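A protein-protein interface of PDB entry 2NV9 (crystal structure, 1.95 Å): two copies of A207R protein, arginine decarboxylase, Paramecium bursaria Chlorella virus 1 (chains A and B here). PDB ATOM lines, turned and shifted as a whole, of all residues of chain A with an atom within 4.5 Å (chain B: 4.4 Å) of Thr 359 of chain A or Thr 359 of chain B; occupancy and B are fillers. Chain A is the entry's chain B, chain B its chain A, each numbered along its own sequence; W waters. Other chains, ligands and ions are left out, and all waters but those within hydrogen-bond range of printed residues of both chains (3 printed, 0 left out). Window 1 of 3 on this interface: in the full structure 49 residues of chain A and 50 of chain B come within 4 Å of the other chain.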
ATOM      1  N   TYR A 287       1.460   1.586  12.509  1.00  0.00           N
ATOM      2  CA  TYR A 287       0.981   2.199  13.734  1.00  0.00           C
ATOM      3  C   TYR A 287       2.141   2.692  14.601  1.00  0.00           C
ATOM      4  O   TYR A 287       1.903   3.272  15.666  1.00  0.00           O
ATOM      5  CB  TYR A 287       0.150   1.174  14.536  1.00  0.00           C
ATOM      6  CG  TYR A 287      -1.154   0.838  13.846  1.00  0.00           C
ATOM      7  CD1 TYR A 287      -2.218   1.736  13.881  1.00  0.00           C
ATOM      8  CD2 TYR A 287      -1.336  -0.374  13.168  1.00  0.00           C
ATOM      9  CE1 TYR A 287      -3.440   1.458  13.225  1.00  0.00           C
ATOM     10  CE2 TYR A 287      -2.563  -0.666  12.535  1.00  0.00           C
ATOM     11  CZ  TYR A 287      -3.616   0.254  12.590  1.00  0.00           C
ATOM     12  OH  TYR A 287      -4.839  -0.017  11.952  1.00  0.00           O
ATOM     13  N   LEU A 357       4.086  10.379  14.789  1.00  0.00           N
ATOM     14  CA  LEU A 357       2.831   9.676  14.577  1.00  0.00           C
ATOM     15  C   LEU A 357       2.746   8.290  15.255  1.00  0.00           C
ATOM     16  O   LEU A 357       1.816   7.507  14.992  1.00  0.00           O
ATOM     17  CB  LEU A 357       2.542   9.617  13.075  1.00  0.00           C
ATOM     18  CG  LEU A 357       2.106  10.994  12.538  1.00  0.00           C
ATOM     19  CD1 LEU A 357       2.314  11.154  11.029  1.00  0.00           C
ATOM     20  CD2 LEU A 357       0.651  11.223  12.856  1.00  0.00           C
ATOM     21  N   THR A 358       3.682   8.007  16.151  1.00  0.00           N
ATOM     22  CA  THR A 358       3.709   6.685  16.801  1.00  0.00           C
ATOM     23  C   THR A 358       2.487   6.477  17.716  1.00  0.00           C
ATOM     24  O   THR A 358       1.982   7.418  18.336  1.00  0.00           O
ATOM     25  CB  THR A 358       4.981   6.439  17.628  1.00  0.00           C
ATOM     26  OG1 THR A 358       5.014   7.354  18.681  1.00  0.00           O
ATOM     27  CG2 THR A 358       6.223   6.634  16.824  1.00  0.00           C
ATOM     28  N   THR A 359       1.991   5.239  17.720  1.00  0.00           N
ATOM     29  CA  THR A 359       0.963   4.783  18.683  1.00  0.00           C
ATOM     30  C   THR A 359       1.499   3.609  19.538  1.00  0.00           C
ATOM     31  O   THR A 359       2.488   2.959  19.200  1.00  0.00           O
ATOM     32  CB  THR A 359      -0.362   4.325  18.028  1.00  0.00           C
ATOM     33  OG1 THR A 359      -0.205   2.993  17.507  1.00  0.00           O
ATOM     34  CG2 THR A 359      -0.820   5.288  16.875  1.00  0.00           C
ATOM     35  N   SER A 360       0.835   3.339  20.662  1.00  0.00           N
ATOM     36  CA  SER A 360       1.165   2.136  21.406  1.00  0.00           C
ATOM     37  C   SER A 360       0.187   0.953  21.101  1.00  0.00           C
ATOM     38  O   SER A 360       0.000   0.014  21.909  1.00  0.00           O
ATOM     39  CB  SER A 360       1.237   2.444  22.881  1.00  0.00           C
ATOM     40  OG  SER A 360      -0.022   2.876  23.351  1.00  0.00           O
ATOM     41  N   PHE A 361      -0.439   1.018  19.934  1.00  0.00           N
ATOM     42  CA  PHE A 361      -1.410  -0.035  19.519  1.00  0.00           C
ATOM     43  C   PHE A 361      -0.766  -1.441  19.603  1.00  0.00           C
ATOM     44  O   PHE A 361       0.393  -1.630  19.225  1.00  0.00           O
ATOM     45  CB  PHE A 361      -1.970   0.269  18.107  1.00  0.00           C
ATOM     46  CG  PHE A 361      -3.108  -0.640  17.670  1.00  0.00           C
ATOM     47  CD1 PHE A 361      -4.175  -0.945  18.539  1.00  0.00           C
ATOM     48  CD2 PHE A 361      -3.151  -1.124  16.355  1.00  0.00           C
ATOM     49  CE1 PHE A 361      -5.209  -1.765  18.134  1.00  0.00           C
ATOM     50  CE2 PHE A 361      -4.198  -1.951  15.925  1.00  0.00           C
ATOM     51  CZ  PHE A 361      -5.221  -2.294  16.824  1.00  0.00           C
ATOM     52  N   PHE A 364       2.853  -2.321  20.963  1.00  0.00           N
ATOM     53  CA  PHE A 364       4.096  -2.021  20.253  1.00  0.00           C
ATOM     54  C   PHE A 364       4.381  -0.491  20.219  1.00  0.00           C
ATOM     55  O   PHE A 364       3.787   0.263  20.995  1.00  0.00           O
ATOM     56  CB  PHE A 364       4.090  -2.668  18.848  1.00  0.00           C
ATOM     57  CG  PHE A 364       3.929  -4.191  18.867  1.00  0.00           C
ATOM     58  CD1 PHE A 364       4.941  -5.018  19.365  1.00  0.00           C
ATOM     59  CD2 PHE A 364       2.786  -4.788  18.338  1.00  0.00           C
ATOM     60  CE1 PHE A 364       4.812  -6.418  19.340  1.00  0.00           C
ATOM     61  CE2 PHE A 364       2.634  -6.145  18.310  1.00  0.00           C
ATOM     62  CZ  PHE A 364       3.641  -6.983  18.829  1.00  0.00           C
ATOM     63  N   GLY A 365       5.222  -0.031  19.290  1.00  0.00           N
ATOM     64  CA  GLY A 365       5.434   1.394  19.088  1.00  0.00           C
ATOM     65  C   GLY A 365       6.625   2.022  19.800  1.00  0.00           C
ATOM     66  O   GLY A 365       6.903   3.233  19.615  1.00  0.00           O
ATOM     67  N   TYR B 287      -6.390  11.716  14.492  1.00  0.00           N
ATOM     68  CA  TYR B 287      -5.122  11.348  15.104  1.00  0.00           C
ATOM     69  C   TYR B 287      -5.231  11.182  16.635  1.00  0.00           C
ATOM     70  O   TYR B 287      -4.211  10.918  17.319  1.00  0.00           O
ATOM     71  CB  TYR B 287      -4.073  12.403  14.758  1.00  0.00           C
ATOM     72  CG  TYR B 287      -3.756  12.416  13.267  1.00  0.00           C
ATOM     73  CD1 TYR B 287      -2.887  11.475  12.727  1.00  0.00           C
ATOM     74  CD2 TYR B 287      -4.315  13.369  12.414  1.00  0.00           C
ATOM     75  CE1 TYR B 287      -2.527  11.500  11.385  1.00  0.00           C
ATOM     76  CE2 TYR B 287      -3.974  13.399  11.044  1.00  0.00           C
ATOM     77  CZ  TYR B 287      -3.103  12.451  10.545  1.00  0.00           C
ATOM     78  OH  TYR B 287      -2.774  12.407   9.212  1.00  0.00           O
ATOM     79  N   LEU B 357      -5.545   3.994  19.983  1.00  0.00           N
ATOM     80  CA  LEU B 357      -4.925   4.515  18.778  1.00  0.00           C
ATOM     81  C   LEU B 357      -4.539   6.019  18.833  1.00  0.00           C
ATOM     82  O   LEU B 357      -4.215   6.630  17.821  1.00  0.00           O
ATOM     83  CB  LEU B 357      -5.820   4.201  17.567  1.00  0.00           C
ATOM     84  CG  LEU B 357      -5.880   2.697  17.241  1.00  0.00           C
ATOM     85  CD1 LEU B 357      -7.050   2.318  16.297  1.00  0.00           C
ATOM     86  CD2 LEU B 357      -4.564   2.282  16.601  1.00  0.00           C
ATOM     87  N   THR B 358      -4.514   6.577  20.038  1.00  0.00           N
ATOM     88  CA  THR B 358      -4.153   8.002  20.198  1.00  0.00           C
ATOM     89  C   THR B 358      -2.708   8.307  19.809  1.00  0.00           C
ATOM     90  O   THR B 358      -1.814   7.525  20.105  1.00  0.00           O
ATOM     91  CB  THR B 358      -4.430   8.547  21.610  1.00  0.00           C
ATOM     92  OG1 THR B 358      -3.565   7.918  22.557  1.00  0.00           O
ATOM     93  CG2 THR B 358      -5.825   8.300  22.018  1.00  0.00           C
ATOM     94  N   THR B 359      -2.501   9.431  19.128  1.00  0.00           N
ATOM     95  CA  THR B 359      -1.153   9.942  18.853  1.00  0.00           C
ATOM     96  C   THR B 359      -1.044  11.330  19.514  1.00  0.00           C
ATOM     97  O   THR B 359      -2.069  11.944  19.874  1.00  0.00           O
ATOM     98  CB  THR B 359      -0.846  10.109  17.315  1.00  0.00           C
ATOM     99  OG1 THR B 359      -1.484  11.297  16.828  1.00  0.00           O
ATOM    100  CG2 THR B 359      -1.263   8.870  16.496  1.00  0.00           C
ATOM    101  N   SER B 360       0.187  11.838  19.632  1.00  0.00           N
ATOM    102  CA  SER B 360       0.393  13.230  20.053  1.00  0.00           C
ATOM    103  C   SER B 360       0.740  14.142  18.829  1.00  0.00           C
ATOM    104  O   SER B 360       1.366  15.179  18.959  1.00  0.00           O
ATOM    105  CB  SER B 360       1.417  13.353  21.197  1.00  0.00           C
ATOM    106  OG  SER B 360       2.672  12.816  20.806  1.00  0.00           O
ATOM    107  N   PHE B 361       0.298  13.737  17.648  1.00  0.00           N
ATOM    108  CA  PHE B 361       0.512  14.547  16.436  1.00  0.00           C
ATOM    109  C   PHE B 361      -0.045  15.991  16.607  1.00  0.00           C
ATOM    110  O   PHE B 361      -1.166  16.191  17.068  1.00  0.00           O
ATOM    111  CB  PHE B 361      -0.108  13.844  15.210  1.00  0.00           C
ATOM    112  CG  PHE B 361       0.211  14.504  13.878  1.00  0.00           C
ATOM    113  CD1 PHE B 361       1.523  14.882  13.550  1.00  0.00           C
ATOM    114  CD2 PHE B 361      -0.790  14.676  12.926  1.00  0.00           C
ATOM    115  CE1 PHE B 361       1.828  15.452  12.304  1.00  0.00           C
ATOM    116  CE2 PHE B 361      -0.509  15.238  11.672  1.00  0.00           C
ATOM    117  CZ  PHE B 361       0.807  15.650  11.376  1.00  0.00           C
ATOM    118  N   PHE B 364      -1.519  17.588  19.929  1.00  0.00           N
ATOM    119  CA  PHE B 364      -2.844  17.275  20.479  1.00  0.00           C
ATOM    120  C   PHE B 364      -2.871  15.843  21.054  1.00  0.00           C
ATOM    121  O   PHE B 364      -1.817  15.268  21.300  1.00  0.00           O
ATOM    122  CB  PHE B 364      -3.958  17.569  19.457  1.00  0.00           C
ATOM    123  CG  PHE B 364      -4.039  19.013  19.045  1.00  0.00           C
ATOM    124  CD1 PHE B 364      -4.395  20.010  19.960  1.00  0.00           C
ATOM    125  CD2 PHE B 364      -3.721  19.394  17.730  1.00  0.00           C
ATOM    126  CE1 PHE B 364      -4.487  21.390  19.555  1.00  0.00           C
ATOM    127  CE2 PHE B 364      -3.802  20.734  17.317  1.00  0.00           C
ATOM    128  CZ  PHE B 364      -4.174  21.744  18.226  1.00  0.00           C
ATOM    129  N   GLY B 365      -4.068  15.281  21.265  1.00  0.00           N
ATOM    130  CA  GLY B 365      -4.224  13.887  21.612  1.00  0.00           C
ATOM    131  C   GLY B 365      -4.464  13.613  23.100  1.00  0.00           C
ATOM    132  O   GLY B 365      -4.662  12.444  23.502  1.00  0.00           O
HETATM  133  O   HOH W   1       1.066   7.452  21.080  1.00  0.00           O
HETATM  134  O   HOH W   2      -1.655   4.916  21.218  1.00  0.00           O
HETATM  135  O   HOH W   3       2.398  10.058  18.590  1.00  0.00           O
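Among the printed residues, merely in contact across the chains: Tyr 287 of chain A with Leu 357 of chain B (3.6 Å), Leu 357 of chain A with Tyr 287 of chain B (3.5 Å), Leu 357 of chain A with Thr 359 of chain B (3.7 Å), Leu 357 of chain A with Phe 361 of chain B (3.5 Å), Thr 359 of chain A with Leu 357 of chain B (3.8 Å), Thr 359 of chain A with Thr 359 of chain B (3.6 Å) and Phe 361 of chain A with Leu 357 of chain B (3.4 Å).
Tyr 287 of chain A touches Leu 357 of chain B, and with the chains exchanged Leu 357 of chain A touches Tyr 287 of chain B.
Leu 357 of chain A touches Thr 359 of chain B, and with the chains exchanged Thr 359 of chain A touches Leu 357 of chain B.
Leu 357 of chain A touches Phe 361 of chain B, and with the chains exchanged Phe 361 of chain A touches Leu 357 of chain B.
Thr 359 of chain B touches its own counterpart, Thr 359 of chain A.
8 positions are printed for both chains.
The side-chain hydroxyl (OG1) of Thr 359 of chain B lies within hydrogen-bond range of the backbone carbonyl oxygen (O) of Tyr 287 of chain B (2.8 Å).
N of Phe 361 of chain B sits at hydrogen-bond distance from OG1 of Thr 359 of chain B, at 3.1 Å.
The side-chain hydroxyl (OG1) of Thr 359 of chain A lies within hydrogen-bond range of the backbone carbonyl oxygen (O) of Tyr 287 of chain A, at 2.8 Å.
OG1 of Thr 359 of chain A lies within hydrogen-bond range of N of Phe 361 of chain A.
Hydrophobic or aromatic side chains of chain B that line the printed part of chain A: Tyr 287, Leu 357 and Phe 361.
Along chain B the printed residues that touch a printed residue of chain A span positions 287 to 361.
Printed residues of chain A that touch a printed residue of chain B: Tyr 287, Leu 357, Thr 359 and Phe 361.
Hydrophobic or aromatic side chains of chain A within 4 Å of the printed part of chain B: Tyr 287, Leu 357 and Phe 361.
Among the printed residues, 7 pairs touch across the chains.
Water W3 bridges O of Thr 358 of chain A and N of Ser 360 of chain B.
Water W2 bridges O of Thr 358 of chain B (2.8 Å) and N of Ser 360 of chain A (3.0 Å).
Water W1 lies within hydrogen-bond range of O of Thr 358 of chain A (2.9 Å) and O of Thr 358 of chain B (3.0 Å).
Of chain B, only Leu 357 and Thr 359 come within 4 Å of Thr 359 of chain A.
Printed residues of chain A within 4 Å of Thr 359 of chain B: Leu 357 (3.7 Å) and Thr 359 (3.6 Å).
Printed residues of chain B within 4 Å of Phe 361 of chain A: Leu 357 (3.4 Å).
Of the printed residues of chain B, Tyr 287 of chain A touches Leu 357.
Of the printed residues of chain A, Leu 357 of chain B touches Tyr 287 (3.6 Å), Thr 359 (3.8 Å) and Phe 361 (3.4 Å).
Printed residues of chain A within 4 Å of Phe 361 of chain B: Leu 357.
Of the printed residues of chain B, Leu 357 of chain A touches Tyr 287 (3.5 Å), Thr 359 (3.7 Å) and Phe 361 (3.5 Å).
Gly 365 of chain B touches none of the printed residues of chain A.
Phe 364 of chain A touches none of the printed residues of chain B.
The nearest printed residue of chain A that does not touch Tyr 287 of chain B is Thr 359 of chain A (6.6 Å).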
